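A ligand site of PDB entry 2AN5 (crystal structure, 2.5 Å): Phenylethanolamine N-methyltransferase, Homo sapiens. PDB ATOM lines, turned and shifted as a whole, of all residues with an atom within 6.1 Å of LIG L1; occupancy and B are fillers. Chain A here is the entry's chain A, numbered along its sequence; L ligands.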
ATOM      1  N   VAL A  23      20.163  -8.051  26.458  1.00  0.00           N
ATOM      2  CA  VAL A  23      18.859  -8.666  26.074  1.00  0.00           C
ATOM      3  C   VAL A  23      17.763  -8.253  27.054  1.00  0.00           C
ATOM      4  O   VAL A  23      16.627  -7.958  26.639  1.00  0.00           O
ATOM      5  CB  VAL A  23      18.956 -10.235  26.054  1.00  0.00           C
ATOM      6  CG1 VAL A  23      20.018 -10.685  25.053  1.00  0.00           C
ATOM      7  CG2 VAL A  23      19.274 -10.769  27.442  1.00  0.00           C
ATOM      8  N   ALA A  24      18.101  -8.222  28.338  1.00  0.00           N
ATOM      9  CA  ALA A  24      17.170  -7.865  29.413  1.00  0.00           C
ATOM     10  C   ALA A  24      16.150  -6.783  29.061  1.00  0.00           C
ATOM     11  O   ALA A  24      14.973  -6.894  29.422  1.00  0.00           O
ATOM     12  CB  ALA A  24      17.957  -7.466  30.661  1.00  0.00           C
ATOM     13  N   TYR A  27      13.325  -7.963  26.595  1.00  0.00           N
ATOM     14  CA  TYR A  27      12.262  -8.728  27.226  1.00  0.00           C
ATOM     15  C   TYR A  27      11.248  -7.847  27.935  1.00  0.00           C
ATOM     16  O   TYR A  27      10.286  -8.349  28.531  1.00  0.00           O
ATOM     17  CB  TYR A  27      12.842  -9.764  28.205  1.00  0.00           C
ATOM     18  CG  TYR A  27      13.146 -11.090  27.544  1.00  0.00           C
ATOM     19  CD1 TYR A  27      14.450 -11.420  27.171  1.00  0.00           C
ATOM     20  CD2 TYR A  27      12.132 -12.006  27.270  1.00  0.00           C
ATOM     21  CE1 TYR A  27      14.725 -12.624  26.535  1.00  0.00           C
ATOM     22  CE2 TYR A  27      12.398 -13.215  26.633  1.00  0.00           C
ATOM     23  CZ  TYR A  27      13.693 -13.512  26.273  1.00  0.00           C
ATOM     24  OH  TYR A  27      13.950 -14.704  25.631  1.00  0.00           O
ATOM     25  N   PHE A  30       8.035  -7.832  25.887  1.00  0.00           N
ATOM     26  CA  PHE A  30       7.527  -9.203  25.784  1.00  0.00           C
ATOM     27  C   PHE A  30       6.014  -9.303  26.034  1.00  0.00           C
ATOM     28  O   PHE A  30       5.551  -8.904  27.103  1.00  0.00           O
ATOM     29  CB  PHE A  30       8.268 -10.066  26.797  1.00  0.00           C
ATOM     30  CG  PHE A  30       8.054 -11.545  26.637  1.00  0.00           C
ATOM     31  CD1 PHE A  30       8.838 -12.274  25.762  1.00  0.00           C
ATOM     32  CD2 PHE A  30       7.090 -12.205  27.395  1.00  0.00           C
ATOM     33  CE1 PHE A  30       8.678 -13.653  25.637  1.00  0.00           C
ATOM     34  CE2 PHE A  30       6.911 -13.578  27.286  1.00  0.00           C
ATOM     35  CZ  PHE A  30       7.706 -14.303  26.402  1.00  0.00           C
ATOM     36  N   TYR A  35       3.135 -14.505  22.659  1.00  0.00           N
ATOM     37  CA  TYR A  35       4.042 -15.623  22.704  1.00  0.00           C
ATOM     38  C   TYR A  35       3.268 -16.948  22.757  1.00  0.00           C
ATOM     39  O   TYR A  35       3.566 -17.883  22.016  1.00  0.00           O
ATOM     40  CB  TYR A  35       4.938 -15.497  23.939  1.00  0.00           C
ATOM     41  CG  TYR A  35       5.837 -16.687  24.161  1.00  0.00           C
ATOM     42  CD1 TYR A  35       7.010 -16.857  23.413  1.00  0.00           C
ATOM     43  CD2 TYR A  35       5.508 -17.651  25.110  1.00  0.00           C
ATOM     44  CE1 TYR A  35       7.839 -17.949  23.624  1.00  0.00           C
ATOM     45  CE2 TYR A  35       6.328 -18.747  25.320  1.00  0.00           C
ATOM     46  CZ  TYR A  35       7.493 -18.885  24.575  1.00  0.00           C
ATOM     47  OH  TYR A  35       8.311 -19.946  24.831  1.00  0.00           O
ATOM     48  N   ASN A  39       3.300 -20.025  19.881  1.00  0.00           N
ATOM     49  CA  ASN A  39       3.871 -21.340  20.161  1.00  0.00           C
ATOM     50  C   ASN A  39       2.999 -22.415  20.740  1.00  0.00           C
ATOM     51  O   ASN A  39       3.377 -23.592  20.689  1.00  0.00           O
ATOM     52  CB  ASN A  39       5.066 -21.156  21.085  1.00  0.00           C
ATOM     53  CG  ASN A  39       6.124 -20.269  20.472  1.00  0.00           C
ATOM     54  OD1 ASN A  39       6.785 -20.664  19.515  1.00  0.00           O
ATOM     55  ND2 ASN A  39       6.273 -19.072  21.019  1.00  0.00           N
ATOM     56  N   TYR A  40       1.861 -22.040  21.305  1.00  0.00           N
ATOM     57  CA  TYR A  40       0.995 -23.049  21.894  1.00  0.00           C
ATOM     58  C   TYR A  40      -0.414 -23.098  21.370  1.00  0.00           C
ATOM     59  O   TYR A  40      -1.279 -23.794  21.927  1.00  0.00           O
ATOM     60  CB  TYR A  40       1.049 -22.914  23.403  1.00  0.00           C
ATOM     61  CG  TYR A  40       2.460 -23.113  23.888  1.00  0.00           C
ATOM     62  CD1 TYR A  40       3.340 -22.035  24.044  1.00  0.00           C
ATOM     63  CD2 TYR A  40       2.984 -24.409  24.042  1.00  0.00           C
ATOM     64  CE1 TYR A  40       4.701 -22.236  24.333  1.00  0.00           C
ATOM     65  CE2 TYR A  40       4.328 -24.620  24.329  1.00  0.00           C
ATOM     66  CZ  TYR A  40       5.175 -23.543  24.468  1.00  0.00           C
ATOM     67  OH  TYR A  40       6.514 -23.775  24.696  1.00  0.00           O
ATOM     68  N   LYS A  57       7.593 -32.996  22.690  1.00  0.00           N
ATOM     69  CA  LYS A  57       8.014 -32.464  23.976  1.00  0.00           C
ATOM     70  C   LYS A  57       7.332 -33.189  25.134  1.00  0.00           C
ATOM     71  O   LYS A  57       7.989 -33.615  26.095  1.00  0.00           O
ATOM     72  CB  LYS A  57       7.721 -30.968  24.052  1.00  0.00           C
ATOM     73  CG  LYS A  57       8.667 -30.095  23.243  1.00  0.00           C
ATOM     74  CD  LYS A  57       8.419 -28.600  23.473  1.00  0.00           C
ATOM     75  CE  LYS A  57       7.041 -28.166  22.995  1.00  0.00           C
ATOM     76  NZ  LYS A  57       6.829 -26.698  23.144  1.00  0.00           N
ATOM     77  N   ASP A  77      11.087 -24.898  38.415  1.00  0.00           N
ATOM     78  CA  ASP A  77      10.979 -24.685  36.981  1.00  0.00           C
ATOM     79  C   ASP A  77      11.611 -23.336  36.678  1.00  0.00           C
ATOM     80  O   ASP A  77      11.080 -22.287  37.042  1.00  0.00           O
ATOM     81  CB  ASP A  77       9.507 -24.702  36.531  1.00  0.00           C
ATOM     82  CG  ASP A  77       9.362 -24.568  35.020  1.00  0.00           C
ATOM     83  OD1 ASP A  77      10.123 -25.223  34.283  1.00  0.00           O
ATOM     84  OD2 ASP A  77       8.474 -23.823  34.557  1.00  0.00           O
ATOM     85  N   ILE A  78      12.753 -23.371  36.004  1.00  0.00           N
ATOM     86  CA  ILE A  78      13.504 -22.171  35.648  1.00  0.00           C
ATOM     87  C   ILE A  78      13.004 -21.509  34.367  1.00  0.00           C
ATOM     88  O   ILE A  78      13.042 -22.118  33.300  1.00  0.00           O
ATOM     89  CB  ILE A  78      15.009 -22.513  35.452  1.00  0.00           C
ATOM     90  CG1 ILE A  78      15.494 -23.417  36.586  1.00  0.00           C
ATOM     91  CG2 ILE A  78      15.823 -21.231  35.374  1.00  0.00           C
ATOM     92  CD1 ILE A  78      15.269 -22.844  37.983  1.00  0.00           C
ATOM     93  N   GLY A  79      12.557 -20.268  34.486  1.00  0.00           N
ATOM     94  CA  GLY A  79      12.079 -19.525  33.320  1.00  0.00           C
ATOM     95  C   GLY A  79      10.779 -20.059  32.757  1.00  0.00           C
ATOM     96  O   GLY A  79      10.650 -20.212  31.536  1.00  0.00           O
ATOM     97  N   SER A  80       9.823 -20.307  33.641  1.00  0.00           N
ATOM     98  CA  SER A  80       8.505 -20.826  33.289  1.00  0.00           C
ATOM     99  C   SER A  80       7.776 -20.033  32.219  1.00  0.00           C
ATOM    100  O   SER A  80       6.965 -20.588  31.468  1.00  0.00           O
ATOM    101  CB  SER A  80       7.618 -20.859  34.534  1.00  0.00           C
ATOM    102  OG  SER A  80       8.190 -21.637  35.560  1.00  0.00           O
ATOM    103  N   GLY A  81       8.024 -18.728  32.157  1.00  0.00           N
ATOM    104  CA  GLY A  81       7.311 -17.920  31.190  1.00  0.00           C
ATOM    105  C   GLY A  81       5.827 -18.036  31.490  1.00  0.00           C
ATOM    106  O   GLY A  81       5.443 -18.207  32.653  1.00  0.00           O
ATOM    107  N   PRO A  82       4.961 -17.936  30.481  1.00  0.00           N
ATOM    108  CA  PRO A  82       3.513 -18.050  30.757  1.00  0.00           C
ATOM    109  C   PRO A  82       2.983 -19.461  30.522  1.00  0.00           C
ATOM    110  O   PRO A  82       1.791 -19.633  30.332  1.00  0.00           O
ATOM    111  CB  PRO A  82       2.917 -17.063  29.762  1.00  0.00           C
ATOM    112  CG  PRO A  82       3.776 -17.299  28.549  1.00  0.00           C
ATOM    113  CD  PRO A  82       5.198 -17.395  29.121  1.00  0.00           C
ATOM    114  N   THR A  83       3.854 -20.459  30.559  1.00  0.00           N
ATOM    115  CA  THR A  83       3.402 -21.816  30.269  1.00  0.00           C
ATOM    116  C   THR A  83       3.465 -22.802  31.425  1.00  0.00           C
ATOM    117  O   THR A  83       4.208 -22.594  32.387  1.00  0.00           O
ATOM    118  CB  THR A  83       4.200 -22.418  29.064  1.00  0.00           C
ATOM    119  OG1 THR A  83       5.533 -22.749  29.494  1.00  0.00           O
ATOM    120  CG2 THR A  83       4.278 -21.411  27.902  1.00  0.00           C
ATOM    121  N   TYR A  85       2.796 -26.547  30.520  1.00  0.00           N
ATOM    122  CA  TYR A  85       2.922 -27.882  29.938  1.00  0.00           C
ATOM    123  C   TYR A  85       4.195 -28.584  30.399  1.00  0.00           C
ATOM    124  O   TYR A  85       4.206 -29.791  30.568  1.00  0.00           O
ATOM    125  CB  TYR A  85       2.910 -27.809  28.402  1.00  0.00           C
ATOM    126  CG  TYR A  85       4.225 -27.329  27.808  1.00  0.00           C
ATOM    127  CD1 TYR A  85       5.272 -28.228  27.585  1.00  0.00           C
ATOM    128  CD2 TYR A  85       4.461 -25.964  27.609  1.00  0.00           C
ATOM    129  CE1 TYR A  85       6.529 -27.760  27.188  1.00  0.00           C
ATOM    130  CE2 TYR A  85       5.709 -25.500  27.212  1.00  0.00           C
ATOM    131  CZ  TYR A  85       6.739 -26.393  27.005  1.00  0.00           C
ATOM    132  OH  TYR A  85       7.981 -25.962  26.632  1.00  0.00           O
ATOM    133  N   GLN A  86       5.259 -27.817  30.595  1.00  0.00           N
ATOM    134  CA  GLN A  86       6.540 -28.387  31.003  1.00  0.00           C
ATOM    135  C   GLN A  86       6.512 -29.082  32.360  1.00  0.00           C
ATOM    136  O   GLN A  86       7.504 -29.700  32.770  1.00  0.00           O
ATOM    137  CB  GLN A  86       7.647 -27.330  31.003  1.00  0.00           C
ATOM    138  CG  GLN A  86       7.464 -26.203  32.012  1.00  0.00           C
ATOM    139  CD  GLN A  86       6.659 -25.039  31.473  1.00  0.00           C
ATOM    140  OE1 GLN A  86       5.870 -25.195  30.533  1.00  0.00           O
ATOM    141  NE2 GLN A  86       6.834 -23.874  32.062  1.00  0.00           N
ATOM    142  N   ASP A 101      10.206 -16.896  36.802  1.00  0.00           N
ATOM    143  CA  ASP A 101      10.313 -16.070  35.615  1.00  0.00           C
ATOM    144  C   ASP A 101      10.732 -14.634  35.875  1.00  0.00           C
ATOM    145  O   ASP A 101      10.359 -14.024  36.874  1.00  0.00           O
ATOM    146  CB  ASP A 101       9.034 -16.073  34.788  1.00  0.00           C
ATOM    147  CG  ASP A 101       9.314 -15.798  33.328  1.00  0.00           C
ATOM    148  OD1 ASP A 101      10.014 -16.642  32.715  1.00  0.00           O
ATOM    149  OD2 ASP A 101       8.873 -14.753  32.800  1.00  0.00           O
ATOM    150  N   PHE A 102      11.497 -14.098  34.923  1.00  0.00           N
ATOM    151  CA  PHE A 102      12.042 -12.758  34.967  1.00  0.00           C
ATOM    152  C   PHE A 102      11.010 -11.651  34.805  1.00  0.00           C
ATOM    153  O   PHE A 102      11.289 -10.495  35.116  1.00  0.00           O
ATOM    154  CB  PHE A 102      13.077 -12.641  33.841  1.00  0.00           C
ATOM    155  CG  PHE A 102      13.829 -11.343  33.820  1.00  0.00           C
ATOM    156  CD1 PHE A 102      14.929 -11.143  34.659  1.00  0.00           C
ATOM    157  CD2 PHE A 102      13.450 -10.326  32.947  1.00  0.00           C
ATOM    158  CE1 PHE A 102      15.633  -9.936  34.624  1.00  0.00           C
ATOM    159  CE2 PHE A 102      14.154  -9.120  32.911  1.00  0.00           C
ATOM    160  CZ  PHE A 102      15.245  -8.925  33.750  1.00  0.00           C
ATOM    161  N   LEU A 103       9.809 -11.977  34.350  1.00  0.00           N
ATOM    162  CA  LEU A 103       8.819 -10.930  34.145  1.00  0.00           C
ATOM    163  C   LEU A 103       7.558 -11.014  34.971  1.00  0.00           C
ATOM    164  O   LEU A 103       6.988 -12.094  35.136  1.00  0.00           O
ATOM    165  CB  LEU A 103       8.407 -10.867  32.675  1.00  0.00           C
ATOM    166  CG  LEU A 103       9.492 -10.537  31.647  1.00  0.00           C
ATOM    167  CD1 LEU A 103       8.872 -10.513  30.255  1.00  0.00           C
ATOM    168  CD2 LEU A 103      10.140  -9.200  31.971  1.00  0.00           C
ATOM    169  N   ASN A 106       4.510 -12.306  32.976  1.00  0.00           N
ATOM    170  CA  ASN A 106       4.415 -13.756  32.845  1.00  0.00           C
ATOM    171  C   ASN A 106       3.888 -14.368  34.128  1.00  0.00           C
ATOM    172  O   ASN A 106       2.927 -15.138  34.088  1.00  0.00           O
ATOM    173  CB  ASN A 106       5.776 -14.378  32.503  1.00  0.00           C
ATOM    174  CG  ASN A 106       6.139 -14.221  31.049  1.00  0.00           C
ATOM    175  OD1 ASN A 106       5.271 -14.258  30.187  1.00  0.00           O
ATOM    176  ND2 ASN A 106       7.429 -14.058  30.763  1.00  0.00           N
ATOM    177  N   ILE A 157      13.180 -14.435  38.911  1.00  0.00           N
ATOM    178  CA  ILE A 157      14.450 -15.129  38.749  1.00  0.00           C
ATOM    179  C   ILE A 157      15.275 -14.512  37.630  1.00  0.00           C
ATOM    180  O   ILE A 157      14.727 -13.938  36.675  1.00  0.00           O
ATOM    181  CB  ILE A 157      14.215 -16.625  38.412  1.00  0.00           C
ATOM    182  CG1 ILE A 157      15.558 -17.357  38.344  1.00  0.00           C
ATOM    183  CG2 ILE A 157      13.466 -16.763  37.085  1.00  0.00           C
ATOM    184  CD1 ILE A 157      15.432 -18.846  38.059  1.00  0.00           C
ATOM    185  N   ASP A 158      16.594 -14.600  37.776  1.00  0.00           N
ATOM    186  CA  ASP A 158      17.520 -14.092  36.779  1.00  0.00           C
ATOM    187  C   ASP A 158      18.677 -15.078  36.696  1.00  0.00           C
ATOM    188  O   ASP A 158      19.544 -15.099  37.568  1.00  0.00           O
ATOM    189  CB  ASP A 158      18.065 -12.732  37.181  1.00  0.00           C
ATOM    190  CG  ASP A 158      18.996 -12.164  36.132  1.00  0.00           C
ATOM    191  OD1 ASP A 158      19.516 -12.948  35.307  1.00  0.00           O
ATOM    192  OD2 ASP A 158      19.200 -10.931  36.116  1.00  0.00           O
ATOM    193  N   VAL A 159      18.679 -15.881  35.646  1.00  0.00           N
ATOM    194  CA  VAL A 159      19.740 -16.867  35.471  1.00  0.00           C
ATOM    195  C   VAL A 159      21.117 -16.231  35.329  1.00  0.00           C
ATOM    196  O   VAL A 159      22.130 -16.930  35.416  1.00  0.00           O
ATOM    197  CB  VAL A 159      19.462 -17.783  34.260  1.00  0.00           C
ATOM    198  CG1 VAL A 159      18.211 -18.603  34.501  1.00  0.00           C
ATOM    199  CG2 VAL A 159      19.301 -16.930  33.004  1.00  0.00           C
ATOM    200  N   HIS A 160      21.154 -14.924  35.121  1.00  0.00           N
ATOM    201  CA  HIS A 160      22.426 -14.210  34.964  1.00  0.00           C
ATOM    202  C   HIS A 160      23.110 -13.964  36.301  1.00  0.00           C
ATOM    203  O   HIS A 160      24.342 -13.878  36.359  1.00  0.00           O
ATOM    204  CB  HIS A 160      22.221 -12.884  34.238  1.00  0.00           C
ATOM    205  CG  HIS A 160      21.715 -13.046  32.840  1.00  0.00           C
ATOM    206  ND1 HIS A 160      22.333 -13.881  31.929  1.00  0.00           N
ATOM    207  CD2 HIS A 160      20.658 -12.496  32.200  1.00  0.00           C
ATOM    208  CE1 HIS A 160      21.669 -13.843  30.795  1.00  0.00           C
ATOM    209  NE2 HIS A 160      20.648 -13.012  30.932  1.00  0.00           N
ATOM    210  N   SER A 180      13.581 -26.891  32.765  1.00  0.00           N
ATOM    211  CA  SER A 180      13.719 -25.615  32.086  1.00  0.00           C
ATOM    212  C   SER A 180      13.484 -25.802  30.592  1.00  0.00           C
ATOM    213  O   SER A 180      14.116 -26.645  29.954  1.00  0.00           O
ATOM    214  CB  SER A 180      15.102 -25.031  32.326  1.00  0.00           C
ATOM    215  OG  SER A 180      15.150 -23.670  31.914  1.00  0.00           O
ATOM    216  N   ALA A 181      12.574 -25.008  30.053  1.00  0.00           N
ATOM    217  CA  ALA A 181      12.241 -25.084  28.644  1.00  0.00           C
ATOM    218  C   ALA A 181      12.346 -23.751  27.938  1.00  0.00           C
ATOM    219  O   ALA A 181      11.680 -22.790  28.310  1.00  0.00           O
ATOM    220  CB  ALA A 181      10.835 -25.661  28.470  1.00  0.00           C
ATOM    221  N   PHE A 182      13.197 -23.697  26.921  1.00  0.00           N
ATOM    222  CA  PHE A 182      13.391 -22.494  26.121  1.00  0.00           C
ATOM    223  C   PHE A 182      13.742 -21.223  26.892  1.00  0.00           C
ATOM    224  O   PHE A 182      13.177 -20.150  26.624  1.00  0.00           O
ATOM    225  CB  PHE A 182      12.134 -22.240  25.274  1.00  0.00           C
ATOM    226  CG  PHE A 182      11.714 -23.431  24.465  1.00  0.00           C
ATOM    227  CD1 PHE A 182      10.716 -24.279  24.927  1.00  0.00           C
ATOM    228  CD2 PHE A 182      12.331 -23.712  23.251  1.00  0.00           C
ATOM    229  CE1 PHE A 182      10.331 -25.404  24.196  1.00  0.00           C
ATOM    230  CE2 PHE A 182      11.958 -24.836  22.501  1.00  0.00           C
ATOM    231  CZ  PHE A 182      10.956 -25.680  22.983  1.00  0.00           C
ATOM    232  N   CYS A 183      14.659 -21.320  27.850  1.00  0.00           N
ATOM    233  CA  CYS A 183      15.048 -20.148  28.615  1.00  0.00           C
ATOM    234  C   CYS A 183      16.484 -19.731  28.378  1.00  0.00           C
ATOM    235  O   CYS A 183      16.744 -18.687  27.763  1.00  0.00           O
ATOM    236  CB  CYS A 183      14.852 -20.374  30.115  1.00  0.00           C
ATOM    237  SG  CYS A 183      15.336 -18.934  31.122  1.00  0.00           S
ATOM    238  N   ALA A 186      17.528 -18.546  25.207  1.00  0.00           N
ATOM    239  CA  ALA A 186      16.683 -17.402  24.838  1.00  0.00           C
ATOM    240  C   ALA A 186      17.021 -16.153  25.642  1.00  0.00           C
ATOM    241  O   ALA A 186      16.376 -15.120  25.478  1.00  0.00           O
ATOM    242  CB  ALA A 186      15.211 -17.755  25.037  1.00  0.00           C
ATOM    243  N   VAL A 187      18.013 -16.244  26.510  1.00  0.00           N
ATOM    244  CA  VAL A 187      18.385 -15.091  27.327  1.00  0.00           C
ATOM    245  C   VAL A 187      19.903 -14.888  27.340  1.00  0.00           C
ATOM    246  O   VAL A 187      20.424 -14.069  28.100  1.00  0.00           O
ATOM    247  CB  VAL A 187      17.890 -15.263  28.788  1.00  0.00           C
ATOM    248  CG1 VAL A 187      16.378 -15.459  28.786  1.00  0.00           C
ATOM    249  CG2 VAL A 187      18.572 -16.454  29.442  1.00  0.00           C
ATOM    250  N   TYR A 222      13.098 -14.863  17.736  1.00  0.00           N
ATOM    251  CA  TYR A 222      11.691 -15.259  17.780  1.00  0.00           C
ATOM    252  C   TYR A 222      10.946 -14.028  18.255  1.00  0.00           C
ATOM    253  O   TYR A 222      11.520 -13.188  18.939  1.00  0.00           O
ATOM    254  CB  TYR A 222      11.480 -16.454  18.720  1.00  0.00           C
ATOM    255  CG  TYR A 222      11.526 -16.146  20.187  1.00  0.00           C
ATOM    256  CD1 TYR A 222      10.367 -15.795  20.875  1.00  0.00           C
ATOM    257  CD2 TYR A 222      12.712 -16.242  20.898  1.00  0.00           C
ATOM    258  CE1 TYR A 222      10.392 -15.573  22.249  1.00  0.00           C
ATOM    259  CE2 TYR A 222      12.760 -16.018  22.276  1.00  0.00           C
ATOM    260  CZ  TYR A 222      11.596 -15.676  22.944  1.00  0.00           C
ATOM    261  OH  TYR A 222      11.627 -15.479  24.303  1.00  0.00           O
HETATM  262  N1  LIG L   1       9.556 -21.934  29.502  1.00  0.00           N
HETATM  263  C1  LIG L   1       8.487 -21.429  28.651  1.00  0.00           C
HETATM  264  C2  LIG L   1       8.803 -19.982  28.206  1.00  0.00           C
HETATM  265  C3  LIG L   1      10.189 -19.747  27.565  1.00  0.00           C
HETATM  266  S1  LIG L   1      10.361 -18.053  26.945  1.00  0.00           S
HETATM  267  C4  LIG L   1       8.204 -22.357  27.451  1.00  0.00           C
HETATM  268  O1  LIG L   1       8.621 -23.539  27.512  1.00  0.00           O
HETATM  269  O2  LIG L   1       7.552 -21.920  26.478  1.00  0.00           O
HETATM  270  C5  LIG L   1      11.822 -17.450  27.839  1.00  0.00           C
HETATM  271  C6  LIG L   1      11.443 -16.928  29.204  1.00  0.00           C
HETATM  272  O3  LIG L   1      12.600 -16.501  29.974  1.00  0.00           O
HETATM  273  C7  LIG L   1      10.437 -15.780  29.257  1.00  0.00           C
HETATM  274  O4  LIG L   1       9.369 -16.111  30.123  1.00  0.00           O
HETATM  275  C8  LIG L   1      11.273 -14.606  29.751  1.00  0.00           C
HETATM  276  O5  LIG L   1      10.516 -13.645  30.467  1.00  0.00           O
HETATM  277  C9  LIG L   1      12.281 -15.309  30.655  1.00  0.00           C
HETATM  278  N2  LIG L   1      13.517 -14.586  30.934  1.00  0.00           N
HETATM  279  C10 LIG L   1      14.018 -13.367  30.359  1.00  0.00           C
HETATM  280  N3  LIG L   1      15.169 -12.983  30.867  1.00  0.00           N
HETATM  281  C11 LIG L   1      15.446 -13.979  31.809  1.00  0.00           C
HETATM  282  C12 LIG L   1      16.545 -14.092  32.681  1.00  0.00           C
HETATM  283  N4  LIG L   1      17.545 -13.214  32.731  1.00  0.00           N
HETATM  284  N5  LIG L   1      16.575 -15.166  33.515  1.00  0.00           N
HETATM  285  C13 LIG L   1      15.543 -16.050  33.469  1.00  0.00           C
HETATM  286  N6  LIG L   1      14.445 -16.030  32.686  1.00  0.00           N
HETATM  287  C14 LIG L   1      14.458 -14.952  31.860  1.00  0.00           C
HETATM  288  O1  LG2 L   2       8.968 -21.123  22.621  1.00  0.00           O
HETATM  289  C1  LG2 L   2      10.010 -21.732  21.851  1.00  0.00           C
HETATM  290  C2  LG2 L   2       9.431 -22.890  21.023  1.00  0.00           C
HETATM  291  C3  LG2 L   2       8.512 -23.752  21.608  1.00  0.00           C
HETATM  292  C4  LG2 L   2       8.019 -24.837  20.900  1.00  0.00           C
HETATM  293  C5  LG2 L   2       8.441 -25.055  19.594  1.00  0.00           C
HETATM  294  C6  LG2 L   2       9.355 -24.184  19.007  1.00  0.00           C
HETATM  295  C7  LG2 L   2       9.851 -23.100  19.706  1.00  0.00           C
HETATM  296  C8  LG2 L   2      10.818 -22.158  18.973  1.00  0.00           C
HETATM  297  C9  LG2 L   2      11.629 -21.310  19.952  1.00  0.00           C
HETATM  298  C10 LG2 L   2      10.694 -20.670  20.987  1.00  0.00           C
HETATM  299  N1  LG2 L   2      11.467 -19.760  21.845  1.00  0.00           N
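The side-chain hydroxyl (OH) of Tyr 40 sits close to the side-chain hydroxyl (OH) of Tyr 85 (3.3 Å). O of Tyr 35 is in hydrogen-bond range of ND2 of Asn 39, at 3.1 Å. OD1 of Asp 101 is in hydrogen-bond range of N of Gly 81, at 2.9 Å. N of His 160 sits at hydrogen-bond distance from OD1 of Asp 158, 2.6 Å away. A ring nitrogen (NE2) of His 160 lies close to the backbone carbonyl oxygen (O) of Val 187, 3.0 Å away. O of Ser 80 lies within hydrogen-bond range of NE2 of Gln 86, at 3.3 Å. The side-chain hydroxyl (OG) of Ser 80 lies within hydrogen-bond range of the side-chain carboxylate (OD2) of Asp 77, 2.4 Å away. The side-chain hydroxyl of Tyr 222 is in hydrogen-bond range of the side-chain hydroxyl of Tyr 27, 2.8 Å away.
The backbone carbonyl oxygen (O) of Phe 182 lies close to a sulfur (S1) of LIG L1, 3.5 Å away. Tyr 27 touches LIG L1. Ser 80 touches LIG L1. CA of Gly 81 touches O4 of LIG L1, at 2.9 Å. Thr 83 touches LIG L1. Phe 102 touches LIG L1 (CB to C14, 3.3 Å). Leu 103 touches LIG L1. Ile 157 touches LIG L1 (O to N5, 3.9 Å). His 160 touches LIG L1. CG1 of Val 187 touches N3 of LIG L1 (3.5 Å). OH of Tyr 222 touches S1 of LIG L1, at 3.9 Å. Of the 32 residues printed, 21 come within 4 Å of LIG L1. Along chain A the residues within 4 Å of LIG L1 span positions 27 to 222.
The backbone carbonyl oxygen (O) of Ala 181 sits at hydrogen-bond distance from a nitrogen (N1) of LIG L1. O1 of LIG L1 sits at hydrogen-bond distance from OH of Tyr 85 (2.7 Å). The side-chain hydroxyl (OH) of Tyr 35 lies within hydrogen-bond range of an oxygen (O2) of LIG L1, 2.7 Å away. An oxygen (O4) of LIG L1 lies within hydrogen-bond range of the side-chain carboxylate of Asp 101. OH of Tyr 40 is in hydrogen-bond range of O2 of LIG L1. The backbone carbonyl oxygen (O) of Gly 79 is in hydrogen-bond range of a nitrogen (N1) of LIG L1 (2.9 Å). O4 of LIG L1 is in hydrogen-bond range of ND2 of Asn 106, at 2.9 Å. N of Val 159 sits at hydrogen-bond distance from N5 of LIG L1. OD1 of Asp 158 is in hydrogen-bond range of N4 of LIG L1. The side-chain sulfur (SG) of Cys 183 is in hydrogen-bond range of a nitrogen (N6) of LIG L1. The side-chain hydroxyl (OH) of Tyr 35 lies within hydrogen-bond range of an oxygen (O1) of LG2 L2.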
